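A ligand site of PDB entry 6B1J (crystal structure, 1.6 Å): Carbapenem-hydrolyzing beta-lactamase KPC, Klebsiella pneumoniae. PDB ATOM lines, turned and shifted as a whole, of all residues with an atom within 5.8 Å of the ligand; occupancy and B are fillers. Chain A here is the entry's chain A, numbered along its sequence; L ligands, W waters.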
ATOM      1  N   LEU A  46      12.136 -18.022 -16.304  1.00  0.00           N
ATOM      2  CA  LEU A  46      11.821 -17.752 -14.895  1.00  0.00           C
ATOM      3  C   LEU A  46      11.267 -16.344 -14.707  1.00  0.00           C
ATOM      4  O   LEU A  46      10.461 -16.112 -13.781  1.00  0.00           O
ATOM      5  CB  LEU A  46      13.097 -17.942 -14.042  1.00  0.00           C
ATOM      6  CG  LEU A  46      13.520 -19.412 -13.891  1.00  0.00           C
ATOM      7  CD1 LEU A  46      14.961 -19.422 -13.431  1.00  0.00           C
ATOM      8  CD2 LEU A  46      12.603 -20.110 -12.903  1.00  0.00           C
ATOM      9  N   CYS A  47      11.768 -15.384 -15.463  1.00  0.00           N
ATOM     10  CA  CYS A  47      11.499 -13.969 -15.196  1.00  0.00           C
ATOM     11  C   CYS A  47      11.802 -13.699 -13.697  1.00  0.00           C
ATOM     12  O   CYS A  47      12.747 -14.291 -13.148  1.00  0.00           O
ATOM     13  CB  CYS A  47      10.069 -13.583 -15.605  1.00  0.00           C
ATOM     14  SG  CYS A  47       9.517 -14.261 -17.172  1.00  0.00           S
ATOM     15  N   SER A  48      11.023 -12.859 -13.033  1.00  0.00           N
ATOM     16  CA  SER A  48      11.253 -12.584 -11.602  1.00  0.00           C
ATOM     17  C   SER A  48      11.074 -13.767 -10.671  1.00  0.00           C
ATOM     18  O   SER A  48      11.404 -13.640  -9.479  1.00  0.00           O
ATOM     19  CB  SER A  48      10.253 -11.550 -11.040  1.00  0.00           C
ATOM     20  OG  SER A  48      10.380 -10.251 -11.596  1.00  0.00           O
ATOM     21  N   SER A  49      10.510 -14.891 -11.144  1.00  0.00           N
ATOM     22  CA  SER A  49      10.193 -15.975 -10.224  1.00  0.00           C
ATOM     23  C   SER A  49      11.426 -16.611  -9.583  1.00  0.00           C
ATOM     24  O   SER A  49      11.322 -17.268  -8.543  1.00  0.00           O
ATOM     25  CB  SER A  49       9.313 -17.022 -10.889  1.00  0.00           C
ATOM     26  OG  SER A  49       9.986 -17.844 -11.821  1.00  0.00           O
ATOM     27  N   LYS A  51      13.424 -15.202  -7.842  1.00  0.00           N
ATOM     28  CA  LYS A  51      13.676 -14.467  -6.600  1.00  0.00           C
ATOM     29  C   LYS A  51      13.236 -15.229  -5.339  1.00  0.00           C
ATOM     30  O   LYS A  51      13.830 -15.043  -4.288  1.00  0.00           O
ATOM     31  CB  LYS A  51      13.032 -13.107  -6.680  1.00  0.00           C
ATOM     32  CG  LYS A  51      13.722 -12.152  -7.668  1.00  0.00           C
ATOM     33  CD  LYS A  51      12.855 -10.926  -7.946  1.00  0.00           C
ATOM     34  CE  LYS A  51      13.464 -10.099  -9.072  1.00  0.00           C
ATOM     35  NZ  LYS A  51      12.558  -9.120  -9.694  1.00  0.00           N
ATOM     36  N   PRO A  82      15.162  -0.148 -12.859  1.00  0.00           N
ATOM     37  CA  PRO A  82      13.699  -0.107 -12.743  1.00  0.00           C
ATOM     38  C   PRO A  82      13.053  -1.311 -12.098  1.00  0.00           C
ATOM     39  O   PRO A  82      13.627  -2.427 -12.114  1.00  0.00           O
ATOM     40  CB  PRO A  82      13.227   0.056 -14.197  1.00  0.00           C
ATOM     41  CG  PRO A  82      14.432   0.624 -14.905  1.00  0.00           C
ATOM     42  CD  PRO A  82      15.619   0.004 -14.255  1.00  0.00           C
ATOM     43  N   TRP A  83      11.872  -1.091 -11.529  1.00  0.00           N
ATOM     44  CA  TRP A  83      11.127  -2.106 -10.743  1.00  0.00           C
ATOM     45  C   TRP A  83      11.945  -2.540  -9.526  1.00  0.00           C
ATOM     46  O   TRP A  83      12.065  -3.747  -9.218  1.00  0.00           O
ATOM     47  CB  TRP A  83      10.678  -3.311 -11.599  1.00  0.00           C
ATOM     48  CG  TRP A  83       9.723  -2.992 -12.666  1.00  0.00           C
ATOM     49  CD1 TRP A  83       8.355  -2.877 -12.563  1.00  0.00           C
ATOM     50  CD2 TRP A  83      10.038  -2.764 -14.050  1.00  0.00           C
ATOM     51  NE1 TRP A  83       7.819  -2.586 -13.808  1.00  0.00           N
ATOM     52  CE2 TRP A  83       8.828  -2.515 -14.734  1.00  0.00           C
ATOM     53  CE3 TRP A  83      11.229  -2.767 -14.782  1.00  0.00           C
ATOM     54  CZ2 TRP A  83       8.782  -2.283 -16.122  1.00  0.00           C
ATOM     55  CZ3 TRP A  83      11.175  -2.505 -16.152  1.00  0.00           C
ATOM     56  CH2 TRP A  83       9.966  -2.260 -16.800  1.00  0.00           C
ATOM     57  N   TYR A 107       7.882  -7.739  -3.247  1.00  0.00           N
ATOM     58  CA  TYR A 107       7.717  -6.617  -4.225  1.00  0.00           C
ATOM     59  C   TYR A 107       8.443  -6.891  -5.545  1.00  0.00           C
ATOM     60  O   TYR A 107       8.414  -6.072  -6.458  1.00  0.00           O
ATOM     61  CB  TYR A 107       8.162  -5.268  -3.597  1.00  0.00           C
ATOM     62  CG  TYR A 107       7.202  -4.875  -2.513  1.00  0.00           C
ATOM     63  CD1 TYR A 107       6.034  -4.138  -2.814  1.00  0.00           C
ATOM     64  CD2 TYR A 107       7.437  -5.244  -1.189  1.00  0.00           C
ATOM     65  CE1 TYR A 107       5.120  -3.807  -1.804  1.00  0.00           C
ATOM     66  CE2 TYR A 107       6.519  -4.937  -0.180  1.00  0.00           C
ATOM     67  CZ  TYR A 107       5.368  -4.228  -0.498  1.00  0.00           C
ATOM     68  OH  TYR A 107       4.495  -3.934   0.512  1.00  0.00           O
ATOM     69  N   SER A 108       9.090  -8.050  -5.653  1.00  0.00           N
ATOM     70  CA  SER A 108       9.814  -8.442  -6.825  1.00  0.00           C
ATOM     71  C   SER A 108      10.908  -7.438  -7.156  1.00  0.00           C
ATOM     72  O   SER A 108      11.183  -7.136  -8.336  1.00  0.00           O
ATOM     73  CB  SER A 108       8.857  -8.659  -7.964  1.00  0.00           C
ATOM     74  OG  SER A 108       9.368  -9.659  -8.808  1.00  0.00           O
ATOM     75  N   ASN A 110      14.000  -5.571  -8.216  1.00  0.00           N
ATOM     76  CA  ASN A 110      15.090  -6.041  -9.088  1.00  0.00           C
ATOM     77  C   ASN A 110      16.484  -5.781  -8.531  1.00  0.00           C
ATOM     78  O   ASN A 110      17.343  -6.675  -8.496  1.00  0.00           O
ATOM     79  CB  ASN A 110      14.959  -5.380 -10.498  1.00  0.00           C
ATOM     80  CG  ASN A 110      13.997  -6.126 -11.410  1.00  0.00           C
ATOM     81  OD1 ASN A 110      13.739  -7.302 -11.223  1.00  0.00           O
ATOM     82  ND2 ASN A 110      13.425  -5.404 -12.390  1.00  0.00           N
ATOM     83  N   GLU A 144      19.333  -9.203 -13.424  1.00  0.00           N
ATOM     84  CA  GLU A 144      18.272  -8.228 -13.739  1.00  0.00           C
ATOM     85  C   GLU A 144      18.905  -7.055 -14.482  1.00  0.00           C
ATOM     86  O   GLU A 144      19.948  -6.537 -14.019  1.00  0.00           O
ATOM     87  CB  GLU A 144      17.539  -7.763 -12.469  1.00  0.00           C
ATOM     88  CG  GLU A 144      16.627  -8.802 -11.850  1.00  0.00           C
ATOM     89  CD  GLU A 144      15.418  -9.139 -12.660  1.00  0.00           C
ATOM     90  OE1 GLU A 144      15.207  -8.540 -13.734  1.00  0.00           O
ATOM     91  OE2 GLU A 144      14.603  -9.981 -12.215  1.00  0.00           O
ATOM     92  N   LEU A 145      18.360  -6.645 -15.629  1.00  0.00           N
ATOM     93  CA  LEU A 145      17.081  -7.080 -16.198  1.00  0.00           C
ATOM     94  C   LEU A 145      17.235  -7.955 -17.453  1.00  0.00           C
ATOM     95  O   LEU A 145      16.222  -8.384 -18.046  1.00  0.00           O
ATOM     96  CB  LEU A 145      16.183  -5.848 -16.539  1.00  0.00           C
ATOM     97  CG  LEU A 145      15.686  -5.127 -15.264  1.00  0.00           C
ATOM     98  CD1 LEU A 145      16.703  -4.172 -14.661  1.00  0.00           C
ATOM     99  CD2 LEU A 145      14.436  -4.387 -15.588  1.00  0.00           C
ATOM    100  N   ASN A 148      15.294 -11.378 -18.396  1.00  0.00           N
ATOM    101  CA  ASN A 148      13.876 -11.376 -18.793  1.00  0.00           C
ATOM    102  C   ASN A 148      13.657 -11.446 -20.280  1.00  0.00           C
ATOM    103  O   ASN A 148      12.506 -11.314 -20.707  1.00  0.00           O
ATOM    104  CB  ASN A 148      13.197 -10.102 -18.274  1.00  0.00           C
ATOM    105  CG  ASN A 148      13.209 -10.028 -16.794  1.00  0.00           C
ATOM    106  OD1 ASN A 148      12.478 -10.765 -16.122  1.00  0.00           O
ATOM    107  ND2 ASN A 148      14.039  -9.152 -16.255  1.00  0.00           N
ATOM    108  N   SER A 149      14.727 -11.580 -21.097  1.00  0.00           N
ATOM    109  CA  SER A 149      14.564 -11.498 -22.561  1.00  0.00           C
ATOM    110  C   SER A 149      13.581 -12.505 -23.146  1.00  0.00           C
ATOM    111  O   SER A 149      12.886 -12.205 -24.125  1.00  0.00           O
ATOM    112  CB  SER A 149      15.920 -11.589 -23.273  1.00  0.00           C
ATOM    113  OG  SER A 149      16.645 -12.706 -22.808  1.00  0.00           O
ATOM    114  N   THR A 194       2.309  -9.305  -5.025  1.00  0.00           N
ATOM    115  CA  THR A 194       2.152  -9.208  -6.485  1.00  0.00           C
ATOM    116  C   THR A 194       1.289 -10.282  -7.100  1.00  0.00           C
ATOM    117  O   THR A 194       1.137 -10.296  -8.335  1.00  0.00           O
ATOM    118  CB  THR A 194       3.531  -9.265  -7.165  1.00  0.00           C
ATOM    119  OG1 THR A 194       4.079 -10.575  -7.032  1.00  0.00           O
ATOM    120  CG2 THR A 194       4.468  -8.237  -6.563  1.00  0.00           C
ATOM    121  N   ARG A 198      -3.293 -14.176  -9.724  1.00  0.00           N
ATOM    122  CA  ARG A 198      -2.727 -15.409 -10.289  1.00  0.00           C
ATOM    123  C   ARG A 198      -3.171 -16.645  -9.512  1.00  0.00           C
ATOM    124  O   ARG A 198      -4.366 -16.856  -9.406  1.00  0.00           O
ATOM    125  CB  ARG A 198      -1.210 -15.207 -10.495  1.00  0.00           C
ATOM    126  CG  ARG A 198      -0.958 -14.228 -11.629  1.00  0.00           C
ATOM    127  CD  ARG A 198       0.497 -13.982 -11.899  1.00  0.00           C
ATOM    128  NE  ARG A 198       0.673 -12.789 -12.678  1.00  0.00           N
ATOM    129  CZ  ARG A 198       1.788 -12.404 -13.296  1.00  0.00           C
ATOM    130  NH1 ARG A 198       2.868 -13.151 -13.282  1.00  0.00           N
ATOM    131  NH2 ARG A 198       1.775 -11.242 -13.960  1.00  0.00           N
ATOM    132  N   LYS A 212       5.281 -16.716  -5.534  1.00  0.00           N
ATOM    133  CA  LYS A 212       6.150 -15.747  -6.202  1.00  0.00           C
ATOM    134  C   LYS A 212       5.815 -15.717  -7.686  1.00  0.00           C
ATOM    135  O   LYS A 212       5.763 -16.784  -8.311  1.00  0.00           O
ATOM    136  CB  LYS A 212       7.616 -16.103  -6.016  1.00  0.00           C
ATOM    137  CG  LYS A 212       8.605 -15.160  -6.724  1.00  0.00           C
ATOM    138  CD  LYS A 212       8.701 -13.818  -6.014  1.00  0.00           C
ATOM    139  CE  LYS A 212       9.330 -12.744  -6.900  1.00  0.00           C
ATOM    140  NZ  LYS A 212       8.345 -12.022  -7.732  1.00  0.00           N
ATOM    141  N   THR A 213       5.682 -14.492  -8.239  1.00  0.00           N
ATOM    142  CA  THR A 213       5.249 -14.277  -9.613  1.00  0.00           C
ATOM    143  C   THR A 213       6.429 -13.901 -10.454  1.00  0.00           C
ATOM    144  O   THR A 213       7.520 -13.578  -9.945  1.00  0.00           O
ATOM    145  CB  THR A 213       4.213 -13.165  -9.678  1.00  0.00           C
ATOM    146  OG1 THR A 213       4.765 -11.997  -9.071  1.00  0.00           O
ATOM    147  CG2 THR A 213       2.991 -13.538  -8.945  1.00  0.00           C
ATOM    148  N   GLY A 214       6.232 -13.978 -11.766  1.00  0.00           N
ATOM    149  CA  GLY A 214       7.187 -13.433 -12.730  1.00  0.00           C
ATOM    150  C   GLY A 214       6.475 -12.927 -13.969  1.00  0.00           C
ATOM    151  O   GLY A 214       5.509 -13.509 -14.391  1.00  0.00           O
ATOM    152  N   THR A 215       6.988 -11.856 -14.565  1.00  0.00           N
ATOM    153  CA  THR A 215       6.370 -11.276 -15.751  1.00  0.00           C
ATOM    154  C   THR A 215       7.495 -10.674 -16.598  1.00  0.00           C
ATOM    155  O   THR A 215       7.958  -9.590 -16.309  1.00  0.00           O
ATOM    156  CB  THR A 215       5.370 -10.156 -15.354  1.00  0.00           C
ATOM    157  OG1 THR A 215       4.424 -10.570 -14.319  1.00  0.00           O
ATOM    158  CG2 THR A 215       4.610  -9.745 -16.620  1.00  0.00           C
ATOM    159  N   CYS A 216       7.944 -11.373 -17.632  1.00  0.00           N
ATOM    160  CA  CYS A 216       9.091 -10.903 -18.433  1.00  0.00           C
ATOM    161  C   CYS A 216       8.769  -9.695 -19.306  1.00  0.00           C
ATOM    162  O   CYS A 216       9.701  -8.990 -19.735  1.00  0.00           O
ATOM    163  CB  CYS A 216       9.610 -12.021 -19.353  1.00  0.00           C
ATOM    164  SG  CYS A 216      10.659 -13.291 -18.602  1.00  0.00           S
ATOM    165  N   GLY A 217       7.492  -9.436 -19.588  1.00  0.00           N
ATOM    166  CA  GLY A 217       7.080  -8.281 -20.389  1.00  0.00           C
ATOM    167  C   GLY A 217       7.125  -8.457 -21.891  1.00  0.00           C
ATOM    168  O   GLY A 217       6.859  -7.478 -22.654  1.00  0.00           O
ATOM    169  N   VAL A 218       7.397  -9.674 -22.333  1.00  0.00           N
ATOM    170  CA  VAL A 218       7.561  -9.999 -23.734  1.00  0.00           C
ATOM    171  C   VAL A 218       7.173 -11.473 -23.922  1.00  0.00           C
ATOM    172  O   VAL A 218       7.107 -12.237 -22.948  1.00  0.00           O
ATOM    173  CB  VAL A 218       9.028  -9.794 -24.241  1.00  0.00           C
ATOM    174  CG1 VAL A 218       9.379  -8.331 -24.344  1.00  0.00           C
ATOM    175  CG2 VAL A 218      10.057 -10.528 -23.409  1.00  0.00           C
ATOM    176  N   ASN A 223       4.370 -16.014 -15.032  1.00  0.00           N
ATOM    177  CA  ASN A 223       4.302 -17.185 -14.217  1.00  0.00           C
ATOM    178  C   ASN A 223       3.928 -16.925 -12.755  1.00  0.00           C
ATOM    179  O   ASN A 223       3.888 -15.775 -12.283  1.00  0.00           O
ATOM    180  CB  ASN A 223       5.625 -17.952 -14.375  1.00  0.00           C
ATOM    181  CG  ASN A 223       6.815 -17.108 -14.042  1.00  0.00           C
ATOM    182  OD1 ASN A 223       6.927 -16.635 -12.925  1.00  0.00           O
ATOM    183  ND2 ASN A 223       7.699 -16.861 -15.014  1.00  0.00           N
HETATM  184  O1  LIG L   1       5.445 -10.401 -11.936  1.00  0.00           O
HETATM  185  S1  LIG L   1       6.294  -9.700 -10.925  1.00  0.00           S
HETATM  186  O2  LIG L   1       7.555 -10.434 -10.704  1.00  0.00           O
HETATM  187  O3  LIG L   1       5.620  -9.304  -9.659  1.00  0.00           O
HETATM  188  O4  LIG L   1       6.612  -8.333 -11.614  1.00  0.00           O
HETATM  189  N1  LIG L   1       7.412  -7.425 -10.802  1.00  0.00           N
HETATM  190  C1  LIG L   1       8.560  -6.756 -11.511  1.00  0.00           C
HETATM  191  C2  LIG L   1       8.033  -6.205 -12.838  1.00  0.00           C
HETATM  192  C3  LIG L   1       7.976  -7.236 -13.875  1.00  0.00           C
HETATM  193  C4  LIG L   1       9.847  -7.583 -11.700  1.00  0.00           C
HETATM  194  N2  LIG L   1       9.669  -8.539 -12.868  1.00  0.00           N
HETATM  195  C5  LIG L   1       9.701  -9.884 -12.695  1.00  0.00           C
HETATM  196  O5  LIG L   1       9.401 -10.729 -13.552  1.00  0.00           O
HETATM  197  C6  LIG L   1       9.362  -7.836 -14.096  1.00  0.00           C
HETATM  198  C7  LIG L   1      10.396  -7.121 -14.730  1.00  0.00           C
HETATM  199  O6  LIG L   1      11.557  -7.085 -14.250  1.00  0.00           O
HETATM  200  N3  LIG L   1      10.025  -6.295 -15.735  1.00  0.00           N
HETATM  201  N4  LIG L   1      10.978  -5.665 -16.472  1.00  0.00           N
HETATM  202  C8  LIG L   1      11.487  -6.404 -17.501  1.00  0.00           C
HETATM  203  O7  LIG L   1      11.343  -7.611 -17.643  1.00  0.00           O
HETATM  204  C9  LIG L   1      12.258  -5.610 -18.589  1.00  0.00           C
HETATM  205  C10 LIG L   1      11.267  -4.703 -19.266  1.00  0.00           C
HETATM  206  C11 LIG L   1      10.190  -5.449 -20.036  1.00  0.00           C
HETATM  207  C12 LIG L   1      10.888  -6.322 -21.098  1.00  0.00           C
HETATM  208  N5  LIG L   1      11.810  -7.245 -20.378  1.00  0.00           N
HETATM  209  C13 LIG L   1      12.878  -6.507 -19.639  1.00  0.00           C
HETATM  210  O   HOH W   1      12.432  -9.821 -13.596  1.00  0.00           O
HETATM  211  O   HOH W   2       2.522 -10.614 -10.749  1.00  0.00           O
HETATM  212  O   HOH W   3       7.905  -6.872 -17.487  1.00  0.00           O
HETATM  213  O   HOH W   4       3.923  -7.334 -10.030  1.00  0.00           O
HETATM  214  O   HOH W   5      15.962  -7.443 -20.889  1.00  0.00           O
HETATM  215  O   HOH W   6      13.693  -8.277 -21.938  1.00  0.00           O
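The backbone NH (N) of Ser 48 lies within hydrogen-bond range of an oxygen (O5) of the ligand. The side-chain hydroxyl (OG) of Ser 48 is bonded to a carbon (C5) of the ligand, at 1.3 Å. O5 of the ligand is in hydrogen-bond range of N of Thr 215 (2.8 Å). An oxygen (O1) of the ligand is in hydrogen-bond range of the side-chain hydroxyl (OG1) of Thr 215. The side-chain hydroxyl (OG) of Ser 108 sits at hydrogen-bond distance from an oxygen (O2) of the ligand, 2.7 Å away. The backbone carbonyl oxygen (O) of Cys 216 lies within hydrogen-bond range of a nitrogen (N5) of the ligand (2.8 Å). OG1 of Thr 213 is in hydrogen-bond range of O3 of the ligand (2.9 Å). The side-chain amide nitrogen (ND2) of Asn 110 lies within hydrogen-bond range of an oxygen (O6) of the ligand, 3.1 Å away. O7 of the ligand sits close to ND2 of Asn 148. O3 of the ligand sits close to OG1 of Thr 194 (3.3 Å). The side-chain amino group of Lys 212 lies within salt-bridge range of an oxygen (O2) of the ligand, at 3.5 Å.
The side-chain hydroxyl (OG) of Ser 108 is in hydrogen-bond range of the side-chain hydroxyl (OG) of Ser 48, 3.0 Å away. OG1 of Thr 215 sits at hydrogen-bond distance from NH2 of Arg 198, at 2.8 Å. The side-chain amino group of Lys 212 sits at hydrogen-bond distance from the side-chain hydroxyl of Ser 108. The side-chain hydroxyl of Thr 213 sits at hydrogen-bond distance from the side-chain hydroxyl of Thr 194, at 2.6 Å. O of Thr 213 lies within hydrogen-bond range of N of Ser 49, at 3.5 Å. The side-chain amide oxygen of Asn 110 sits at hydrogen-bond distance from the side-chain amino group of Lys 51 (2.7 Å). The backbone carbonyl oxygen of Pro 82 lies within hydrogen-bond range of the side-chain amide nitrogen of Asn 110 (3.0 Å). O of Gly 214 is in hydrogen-bond range of N of Asn 223, at 2.8 Å.
Residues that only touch the ligand: Cys 47 (3.6 Å), Lys 51 (3.7 Å), Trp 83 (3.2 Å), Glu 144 (3.96 Å), Leu 145 (3.8 Å) and Gly 214 (3.4 Å). Hydrophobic or aromatic side chains that line the ligand: Trp 83 and Leu 145.
Water W6 lies within hydrogen-bond range of N5 of the ligand and O of Asn 148. Water W3 lies within hydrogen-bond range of a nitrogen (N3) of the ligand (2.8 Å), the backbone carbonyl oxygen (O) of Thr 215 (3.0 Å) and the backbone NH (N) of Gly 217 (3.3 Å). Water W2 lies within hydrogen-bond range of O of Thr 194, OG1 of Thr 213, O1 of the ligand and NH2 of Arg 198.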
